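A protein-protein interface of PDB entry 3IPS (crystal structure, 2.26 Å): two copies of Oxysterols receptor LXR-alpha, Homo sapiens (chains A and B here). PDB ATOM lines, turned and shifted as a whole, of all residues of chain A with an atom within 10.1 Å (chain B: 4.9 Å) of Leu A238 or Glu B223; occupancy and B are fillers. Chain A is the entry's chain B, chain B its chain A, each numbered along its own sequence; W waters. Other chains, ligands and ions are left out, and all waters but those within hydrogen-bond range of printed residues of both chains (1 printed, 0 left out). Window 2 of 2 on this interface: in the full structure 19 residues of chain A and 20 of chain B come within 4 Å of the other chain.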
ATOM      1  N   LEU A 185      21.095  18.581 -17.810  1.00  0.00           N
ATOM      2  CA  LEU A 185      21.114  19.809 -17.003  1.00  0.00           C
ATOM      3  C   LEU A 185      19.749  20.141 -16.355  1.00  0.00           C
ATOM      4  O   LEU A 185      19.668  20.990 -15.457  1.00  0.00           O
ATOM      5  CB  LEU A 185      21.515  21.010 -17.872  1.00  0.00           C
ATOM      6  CG  LEU A 185      22.895  21.092 -18.502  1.00  0.00           C
ATOM      7  CD1 LEU A 185      23.102  22.487 -18.992  1.00  0.00           C
ATOM      8  CD2 LEU A 185      23.950  20.707 -17.506  1.00  0.00           C
ATOM      9  N   LEU A 187      17.096  22.041 -16.950  1.00  0.00           N
ATOM     10  CA  LEU A 187      16.767  23.467 -16.742  1.00  0.00           C
ATOM     11  C   LEU A 187      15.274  23.614 -16.518  1.00  0.00           C
ATOM     12  O   LEU A 187      14.496  22.776 -16.976  1.00  0.00           O
ATOM     13  CB  LEU A 187      17.169  24.334 -17.941  1.00  0.00           C
ATOM     14  CG  LEU A 187      18.598  24.264 -18.456  1.00  0.00           C
ATOM     15  CD1 LEU A 187      18.799  25.359 -19.485  1.00  0.00           C
ATOM     16  CD2 LEU A 187      19.589  24.411 -17.345  1.00  0.00           C
ATOM     17  N   LEU A 225      20.663  35.564 -15.101  1.00  0.00           N
ATOM     18  CA  LEU A 225      20.875  34.125 -15.080  1.00  0.00           C
ATOM     19  C   LEU A 225      21.827  33.716 -13.964  1.00  0.00           C
ATOM     20  O   LEU A 225      21.570  32.756 -13.251  1.00  0.00           O
ATOM     21  CB  LEU A 225      21.416  33.620 -16.420  1.00  0.00           C
ATOM     22  CG  LEU A 225      21.576  32.094 -16.537  1.00  0.00           C
ATOM     23  CD1 LEU A 225      20.245  31.417 -16.257  1.00  0.00           C
ATOM     24  CD2 LEU A 225      22.130  31.642 -17.889  1.00  0.00           C
ATOM     25  N   HIS A 226      22.937  34.431 -13.816  1.00  0.00           N
ATOM     26  CA  HIS A 226      23.922  34.076 -12.784  1.00  0.00           C
ATOM     27  C   HIS A 226      23.224  34.078 -11.450  1.00  0.00           C
ATOM     28  O   HIS A 226      23.277  33.088 -10.717  1.00  0.00           O
ATOM     29  CB  HIS A 226      25.070  35.079 -12.761  1.00  0.00           C
ATOM     30  CG  HIS A 226      26.190  34.717 -11.831  1.00  0.00           C
ATOM     31  ND1 HIS A 226      27.496  35.089 -12.078  1.00  0.00           N
ATOM     32  CD2 HIS A 226      26.211  34.023 -10.665  1.00  0.00           C
ATOM     33  CE1 HIS A 226      28.271  34.636 -11.106  1.00  0.00           C
ATOM     34  NE2 HIS A 226      27.516  33.992 -10.233  1.00  0.00           N
ATOM     35  N   VAL A 229      20.469  31.292 -10.965  1.00  0.00           N
ATOM     36  CA  VAL A 229      20.997  29.943 -10.821  1.00  0.00           C
ATOM     37  C   VAL A 229      21.674  29.719  -9.473  1.00  0.00           C
ATOM     38  O   VAL A 229      21.804  28.582  -9.058  1.00  0.00           O
ATOM     39  CB  VAL A 229      21.952  29.603 -11.982  1.00  0.00           C
ATOM     40  CG1 VAL A 229      22.592  28.265 -11.774  1.00  0.00           C
ATOM     41  CG2 VAL A 229      21.191  29.622 -13.304  1.00  0.00           C
ATOM     42  N   SER A 230      22.100  30.790  -8.794  1.00  0.00           N
ATOM     43  CA  SER A 230      22.644  30.698  -7.419  1.00  0.00           C
ATOM     44  C   SER A 230      21.574  30.402  -6.355  1.00  0.00           C
ATOM     45  O   SER A 230      21.894  30.035  -5.217  1.00  0.00           O
ATOM     46  CB  SER A 230      23.322  32.012  -7.053  1.00  0.00           C
ATOM     47  OG  SER A 230      24.227  32.371  -8.065  1.00  0.00           O
ATOM     48  N   HIS A 233      20.376  26.534  -7.799  1.00  0.00           N
ATOM     49  CA  HIS A 233      21.488  25.600  -7.615  1.00  0.00           C
ATOM     50  C   HIS A 233      22.541  26.177  -6.658  1.00  0.00           C
ATOM     51  O   HIS A 233      23.655  26.545  -7.085  1.00  0.00           O
ATOM     52  CB  HIS A 233      22.141  25.275  -8.971  1.00  0.00           C
ATOM     53  CG  HIS A 233      21.315  24.380  -9.829  1.00  0.00           C
ATOM     54  ND1 HIS A 233      21.081  23.062  -9.509  1.00  0.00           N
ATOM     55  CD2 HIS A 233      20.652  24.615 -10.985  1.00  0.00           C
ATOM     56  CE1 HIS A 233      20.302  22.523 -10.432  1.00  0.00           C
ATOM     57  NE2 HIS A 233      20.018  23.449 -11.334  1.00  0.00           N
ATOM     58  N   PRO A 234      22.216  26.232  -5.354  1.00  0.00           N
ATOM     59  CA  PRO A 234      23.096  26.905  -4.388  1.00  0.00           C
ATOM     60  C   PRO A 234      24.412  26.174  -4.070  1.00  0.00           C
ATOM     61  O   PRO A 234      25.312  26.810  -3.514  1.00  0.00           O
ATOM     62  CB  PRO A 234      22.227  27.003  -3.131  1.00  0.00           C
ATOM     63  CG  PRO A 234      21.269  25.865  -3.245  1.00  0.00           C
ATOM     64  CD  PRO A 234      21.007  25.677  -4.709  1.00  0.00           C
ATOM     65  N   HIS A 235      24.528  24.875  -4.403  1.00  0.00           N
ATOM     66  CA  HIS A 235      25.761  24.117  -4.116  1.00  0.00           C
ATOM     67  C   HIS A 235      26.604  23.790  -5.338  1.00  0.00           C
ATOM     68  O   HIS A 235      27.817  23.670  -5.213  1.00  0.00           O
ATOM     69  CB  HIS A 235      25.448  22.851  -3.325  1.00  0.00           C
ATOM     70  CG  HIS A 235      24.654  23.116  -2.081  1.00  0.00           C
ATOM     71  ND1 HIS A 235      25.212  23.664  -0.945  1.00  0.00           N
ATOM     72  CD2 HIS A 235      23.334  22.953  -1.815  1.00  0.00           C
ATOM     73  CE1 HIS A 235      24.271  23.806  -0.025  1.00  0.00           C
ATOM     74  NE2 HIS A 235      23.122  23.387  -0.530  1.00  0.00           N
ATOM     75  N   ASP A 236      25.989  23.665  -6.516  1.00  0.00           N
ATOM     76  CA  ASP A 236      26.761  23.447  -7.759  1.00  0.00           C
ATOM     77  C   ASP A 236      27.034  24.780  -8.460  1.00  0.00           C
ATOM     78  O   ASP A 236      26.202  25.258  -9.238  1.00  0.00           O
ATOM     79  CB  ASP A 236      26.031  22.462  -8.689  1.00  0.00           C
ATOM     80  CG  ASP A 236      26.897  21.983  -9.836  1.00  0.00           C
ATOM     81  OD1 ASP A 236      28.116  22.233  -9.826  1.00  0.00           O
ATOM     82  OD2 ASP A 236      26.362  21.366 -10.772  1.00  0.00           O
ATOM     83  N   ARG A 237      28.200  25.371  -8.173  1.00  0.00           N
ATOM     84  CA  ARG A 237      28.646  26.637  -8.801  1.00  0.00           C
ATOM     85  C   ARG A 237      28.958  26.506 -10.304  1.00  0.00           C
ATOM     86  O   ARG A 237      29.126  27.516 -11.011  1.00  0.00           O
ATOM     87  CB  ARG A 237      29.875  27.222  -8.080  1.00  0.00           C
ATOM     88  CG  ARG A 237      29.577  28.356  -7.075  1.00  0.00           C
ATOM     89  CD  ARG A 237      30.738  29.427  -7.018  1.00  0.00           C
ATOM     90  NE  ARG A 237      30.316  30.780  -6.576  1.00  0.00           N
ATOM     91  CZ  ARG A 237      29.527  31.631  -7.265  1.00  0.00           C
ATOM     92  NH1 ARG A 237      29.012  31.308  -8.461  1.00  0.00           N
ATOM     93  NH2 ARG A 237      29.238  32.826  -6.744  1.00  0.00           N
ATOM     94  N   LEU A 238      29.021  25.260 -10.777  1.00  0.00           N
ATOM     95  CA  LEU A 238      29.209  24.937 -12.197  1.00  0.00           C
ATOM     96  C   LEU A 238      27.953  25.009 -13.052  1.00  0.00           C
ATOM     97  O   LEU A 238      28.056  24.933 -14.276  1.00  0.00           O
ATOM     98  CB  LEU A 238      29.778  23.531 -12.348  1.00  0.00           C
ATOM     99  CG  LEU A 238      31.297  23.457 -12.234  1.00  0.00           C
ATOM    100  CD1 LEU A 238      31.690  22.076 -11.707  1.00  0.00           C
ATOM    101  CD2 LEU A 238      31.948  23.766 -13.591  1.00  0.00           C
ATOM    102  N   MET A 239      26.773  25.112 -12.449  1.00  0.00           N
ATOM    103  CA  MET A 239      25.556  25.047 -13.257  1.00  0.00           C
ATOM    104  C   MET A 239      25.408  26.274 -14.112  1.00  0.00           C
ATOM    105  O   MET A 239      24.928  26.192 -15.221  1.00  0.00           O
ATOM    106  CB  MET A 239      24.315  24.872 -12.390  1.00  0.00           C
ATOM    107  CG  MET A 239      24.124  23.448 -11.858  1.00  0.00           C
ATOM    108  SD  MET A 239      24.193  22.132 -13.103  1.00  0.00           S
ATOM    109  CE  MET A 239      22.792  22.513 -14.169  1.00  0.00           C
ATOM    110  N   PHE A 240      25.792  27.424 -13.587  1.00  0.00           N
ATOM    111  CA  PHE A 240      25.767  28.644 -14.381  1.00  0.00           C
ATOM    112  C   PHE A 240      26.639  28.444 -15.624  1.00  0.00           C
ATOM    113  O   PHE A 240      26.091  28.460 -16.724  1.00  0.00           O
ATOM    114  CB  PHE A 240      26.168  29.867 -13.547  1.00  0.00           C
ATOM    115  CG  PHE A 240      26.419  31.116 -14.354  1.00  0.00           C
ATOM    116  CD1 PHE A 240      25.448  31.630 -15.182  1.00  0.00           C
ATOM    117  CD2 PHE A 240      27.635  31.791 -14.257  1.00  0.00           C
ATOM    118  CE1 PHE A 240      25.686  32.801 -15.927  1.00  0.00           C
ATOM    119  CE2 PHE A 240      27.876  32.960 -14.996  1.00  0.00           C
ATOM    120  CZ  PHE A 240      26.895  33.462 -15.832  1.00  0.00           C
ATOM    121  N   PRO A 241      27.973  28.232 -15.469  1.00  0.00           N
ATOM    122  CA  PRO A 241      28.829  28.059 -16.663  1.00  0.00           C
ATOM    123  C   PRO A 241      28.413  26.910 -17.554  1.00  0.00           C
ATOM    124  O   PRO A 241      28.422  27.073 -18.755  1.00  0.00           O
ATOM    125  CB  PRO A 241      30.223  27.801 -16.095  1.00  0.00           C
ATOM    126  CG  PRO A 241      30.009  27.444 -14.707  1.00  0.00           C
ATOM    127  CD  PRO A 241      28.773  28.160 -14.242  1.00  0.00           C
ATOM    128  N   ARG A 242      28.030  25.767 -16.996  1.00  0.00           N
ATOM    129  CA  ARG A 242      27.537  24.672 -17.833  1.00  0.00           C
ATOM    130  C   ARG A 242      26.405  25.102 -18.768  1.00  0.00           C
ATOM    131  O   ARG A 242      26.284  24.588 -19.871  1.00  0.00           O
ATOM    132  CB  ARG A 242      27.077  23.498 -16.992  1.00  0.00           C
ATOM    133  CG  ARG A 242      28.201  22.659 -16.480  1.00  0.00           C
ATOM    134  CD  ARG A 242      27.666  21.579 -15.593  1.00  0.00           C
ATOM    135  NE  ARG A 242      26.987  20.535 -16.349  1.00  0.00           N
ATOM    136  CZ  ARG A 242      26.536  19.402 -15.812  1.00  0.00           C
ATOM    137  NH1 ARG A 242      26.663  19.187 -14.505  1.00  0.00           N
ATOM    138  NH2 ARG A 242      25.949  18.491 -16.568  1.00  0.00           N
ATOM    139  N   MET A 243      25.582  26.048 -18.332  1.00  0.00           N
ATOM    140  CA  MET A 243      24.499  26.544 -19.189  1.00  0.00           C
ATOM    141  C   MET A 243      24.965  27.470 -20.289  1.00  0.00           C
ATOM    142  O   MET A 243      24.358  27.477 -21.355  1.00  0.00           O
ATOM    143  CB  MET A 243      23.460  27.300 -18.371  1.00  0.00           C
ATOM    144  CG  MET A 243      22.520  26.398 -17.625  1.00  0.00           C
ATOM    145  SD  MET A 243      21.546  27.380 -16.533  1.00  0.00           S
ATOM    146  CE  MET A 243      21.387  26.196 -15.168  1.00  0.00           C
ATOM    147  N   LEU A 244      25.983  28.291 -20.016  1.00  0.00           N
ATOM    148  CA  LEU A 244      26.506  29.234 -21.017  1.00  0.00           C
ATOM    149  C   LEU A 244      27.269  28.481 -22.098  1.00  0.00           C
ATOM    150  O   LEU A 244      27.195  28.824 -23.262  1.00  0.00           O
ATOM    151  CB  LEU A 244      27.454  30.265 -20.384  1.00  0.00           C
ATOM    152  CG  LEU A 244      26.871  31.303 -19.446  1.00  0.00           C
ATOM    153  CD1 LEU A 244      27.971  32.279 -19.058  1.00  0.00           C
ATOM    154  CD2 LEU A 244      25.718  32.021 -20.106  1.00  0.00           C
ATOM    155  N   MET A 245      27.998  27.451 -21.686  1.00  0.00           N
ATOM    156  CA  MET A 245      28.770  26.603 -22.601  1.00  0.00           C
ATOM    157  C   MET A 245      27.881  25.911 -23.637  1.00  0.00           C
ATOM    158  O   MET A 245      28.356  25.451 -24.675  1.00  0.00           O
ATOM    159  CB  MET A 245      29.518  25.526 -21.824  1.00  0.00           C
ATOM    160  CG  MET A 245      30.504  26.024 -20.749  1.00  0.00           C
ATOM    161  SD  MET A 245      31.731  27.104 -21.434  1.00  0.00           S
ATOM    162  CE  MET A 245      32.623  26.078 -22.589  1.00  0.00           C
ATOM    163  N   LYS A 246      26.595  25.825 -23.351  1.00  0.00           N
ATOM    164  CA  LYS A 246      25.679  25.232 -24.294  1.00  0.00           C
ATOM    165  C   LYS A 246      25.450  26.144 -25.472  1.00  0.00           C
ATOM    166  O   LYS A 246      25.116  25.663 -26.523  1.00  0.00           O
ATOM    167  CB  LYS A 246      24.371  24.828 -23.597  1.00  0.00           C
ATOM    168  CG  LYS A 246      24.579  23.624 -22.588  1.00  0.00           C
ATOM    169  CD  LYS A 246      24.337  22.224 -23.210  1.00  0.00           C
ATOM    170  CE  LYS A 246      25.400  21.187 -22.829  1.00  0.00           C
ATOM    171  NZ  LYS A 246      26.328  20.906 -23.969  1.00  0.00           N
ATOM    172  N   GLN B  46      43.849  24.330  -7.513  1.00  0.00           N
ATOM    173  CA  GLN B  46      43.605  25.227  -8.644  1.00  0.00           C
ATOM    174  C   GLN B  46      44.790  26.141  -8.856  1.00  0.00           C
ATOM    175  O   GLN B  46      45.143  26.447  -9.994  1.00  0.00           O
ATOM    176  CB  GLN B  46      42.353  26.075  -8.405  1.00  0.00           C
ATOM    177  CG  GLN B  46      41.048  25.276  -8.373  1.00  0.00           C
ATOM    178  CD  GLN B  46      39.870  26.100  -7.901  1.00  0.00           C
ATOM    179  OE1 GLN B  46      39.991  26.895  -6.977  1.00  0.00           O
ATOM    180  NE2 GLN B  46      38.716  25.907  -8.526  1.00  0.00           N
ATOM    181  N   HIS B 219      35.228  21.163 -16.685  1.00  0.00           N
ATOM    182  CA  HIS B 219      34.725  21.839 -15.496  1.00  0.00           C
ATOM    183  C   HIS B 219      35.820  22.240 -14.558  1.00  0.00           C
ATOM    184  O   HIS B 219      35.838  23.341 -14.085  1.00  0.00           O
ATOM    185  CB  HIS B 219      33.727  20.952 -14.771  1.00  0.00           C
ATOM    186  CG  HIS B 219      32.516  20.675 -15.585  1.00  0.00           C
ATOM    187  ND1 HIS B 219      31.702  19.583 -15.373  1.00  0.00           N
ATOM    188  CD2 HIS B 219      32.005  21.336 -16.651  1.00  0.00           C
ATOM    189  CE1 HIS B 219      30.727  19.598 -16.263  1.00  0.00           C
ATOM    190  NE2 HIS B 219      30.892  20.646 -17.055  1.00  0.00           N
ATOM    191  N   THR B 220      36.765  21.356 -14.300  1.00  0.00           N
ATOM    192  CA  THR B 220      37.845  21.712 -13.410  1.00  0.00           C
ATOM    193  C   THR B 220      38.557  22.981 -13.910  1.00  0.00           C
ATOM    194  O   THR B 220      38.954  23.831 -13.110  1.00  0.00           O
ATOM    195  CB  THR B 220      38.860  20.581 -13.272  1.00  0.00           C
ATOM    196  OG1 THR B 220      39.783  20.662 -14.364  1.00  0.00           O
ATOM    197  CG2 THR B 220      38.162  19.216 -13.258  1.00  0.00           C
ATOM    198  N   TYR B 221      38.694  23.140 -15.219  1.00  0.00           N
ATOM    199  CA  TYR B 221      39.316  24.368 -15.748  1.00  0.00           C
ATOM    200  C   TYR B 221      38.392  25.581 -15.683  1.00  0.00           C
ATOM    201  O   TYR B 221      38.832  26.666 -15.334  1.00  0.00           O
ATOM    202  CB  TYR B 221      39.838  24.153 -17.168  1.00  0.00           C
ATOM    203  CG  TYR B 221      40.931  23.127 -17.211  1.00  0.00           C
ATOM    204  CD1 TYR B 221      42.246  23.472 -16.937  1.00  0.00           C
ATOM    205  CD2 TYR B 221      40.652  21.798 -17.486  1.00  0.00           C
ATOM    206  CE1 TYR B 221      43.266  22.506 -16.963  1.00  0.00           C
ATOM    207  CE2 TYR B 221      41.650  20.850 -17.533  1.00  0.00           C
ATOM    208  CZ  TYR B 221      42.958  21.208 -17.263  1.00  0.00           C
ATOM    209  OH  TYR B 221      43.969  20.265 -17.268  1.00  0.00           O
ATOM    210  N   VAL B 222      37.115  25.388 -16.003  1.00  0.00           N
ATOM    211  CA  VAL B 222      36.105  26.448 -15.951  1.00  0.00           C
ATOM    212  C   VAL B 222      35.977  27.003 -14.530  1.00  0.00           C
ATOM    213  O   VAL B 222      35.904  28.214 -14.338  1.00  0.00           O
ATOM    214  CB  VAL B 222      34.733  25.922 -16.411  1.00  0.00           C
ATOM    215  CG1 VAL B 222      33.657  26.963 -16.181  1.00  0.00           C
ATOM    216  CG2 VAL B 222      34.785  25.456 -17.893  1.00  0.00           C
ATOM    217  N   GLU B 223      35.988  26.111 -13.541  1.00  0.00           N
ATOM    218  CA  GLU B 223      36.031  26.506 -12.125  1.00  0.00           C
ATOM    219  C   GLU B 223      37.314  27.231 -11.730  1.00  0.00           C
ATOM    220  O   GLU B 223      37.260  28.181 -10.935  1.00  0.00           O
ATOM    221  CB  GLU B 223      35.895  25.294 -11.201  1.00  0.00           C
ATOM    222  CG  GLU B 223      34.481  25.012 -10.749  1.00  0.00           C
ATOM    223  CD  GLU B 223      34.454  24.437  -9.339  1.00  0.00           C
ATOM    224  OE1 GLU B 223      35.369  23.632  -8.999  1.00  0.00           O
ATOM    225  OE2 GLU B 223      33.527  24.806  -8.560  1.00  0.00           O
ATOM    226  N   ALA B 224      38.453  26.736 -12.230  1.00  0.00           N
ATOM    227  CA  ALA B 224      39.764  27.388 -12.043  1.00  0.00           C
ATOM    228  C   ALA B 224      39.759  28.839 -12.517  1.00  0.00           C
ATOM    229  O   ALA B 224      40.259  29.694 -11.825  1.00  0.00           O
ATOM    230  CB  ALA B 224      40.866  26.611 -12.772  1.00  0.00           C
ATOM    231  N   LEU B 225      39.181  29.080 -13.691  1.00  0.00           N
ATOM    232  CA  LEU B 225      39.064  30.384 -14.309  1.00  0.00           C
ATOM    233  C   LEU B 225      38.129  31.267 -13.526  1.00  0.00           C
ATOM    234  O   LEU B 225      38.370  32.469 -13.384  1.00  0.00           O
ATOM    235  CB  LEU B 225      38.509  30.232 -15.734  1.00  0.00           C
ATOM    236  CG  LEU B 225      38.383  31.502 -16.595  1.00  0.00           C
ATOM    237  CD1 LEU B 225      39.754  32.017 -16.965  1.00  0.00           C
ATOM    238  CD2 LEU B 225      37.524  31.282 -17.852  1.00  0.00           C
ATOM    239  N   HIS B 226      37.030  30.688 -13.058  1.00  0.00           N
ATOM    240  CA  HIS B 226      36.121  31.419 -12.208  1.00  0.00           C
ATOM    241  C   HIS B 226      36.849  31.964 -10.992  1.00  0.00           C
ATOM    242  O   HIS B 226      36.783  33.156 -10.700  1.00  0.00           O
ATOM    243  CB  HIS B 226      34.991  30.511 -11.731  1.00  0.00           C
ATOM    244  CG  HIS B 226      33.776  31.254 -11.280  1.00  0.00           C
ATOM    245  ND1 HIS B 226      32.558  30.635 -11.087  1.00  0.00           N
ATOM    246  CD2 HIS B 226      33.580  32.569 -11.019  1.00  0.00           C
ATOM    247  CE1 HIS B 226      31.673  31.539 -10.708  1.00  0.00           C
ATOM    248  NE2 HIS B 226      32.263  32.719 -10.667  1.00  0.00           N
ATOM    249  N   ALA B 227      37.514  31.069 -10.262  1.00  0.00           N
ATOM    250  CA  ALA B 227      38.191  31.445  -9.032  1.00  0.00           C
ATOM    251  C   ALA B 227      39.228  32.495  -9.337  1.00  0.00           C
ATOM    252  O   ALA B 227      39.328  33.475  -8.635  1.00  0.00           O
ATOM    253  CB  ALA B 227      38.830  30.255  -8.395  1.00  0.00           C
HETATM  254  O   HOH W   1      31.810  27.994 -11.385  1.00  0.00           O
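The side-chain carboxylate (OD1) of Asp A236 lies close to the backbone NH (N) of Leu A238.
Among the printed residues, merely in contact across the chains: Arg A237 with His B226, Leu A238 with His B219, Leu A238 with Glu B223, Pro A241 with Val B222 and Arg A242 with His B219.
Leu A238 touches just these residues of chain B: His B219 (3.5 Å) and Glu B223 (3.8 Å). Val B222 touches just one residue of chain A: Pro A241 (3.5 Å). No residue of chain A comes within 4 Å of Ala B224. Printed residues of chain A within 4 Å of His B226: Arg A237. Printed residues of chain B within 4 Å of Arg A237: His B226.
Hydrophobic or aromatic side chains of chain A that line the printed part of chain B: Leu A238 and Pro A241. Of the 10 printed residues of chain B, 4 touch a printed residue of chain A. Hydrophobic or aromatic side chains of chain B within 4 Å of the printed part of chain A: His B219, Val B222 and His B226. Among the printed residues, 5 pairs touch across the chains.
2 positions are printed for both chains. Of the 5 pairs that touch across the chains among the printed residues, none has its exchanged pair printed and touching as well.
Water W1 lies within hydrogen-bond range of O of Arg A237 (2.8 Å) and ND1 of His B226 (2.8 Å).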
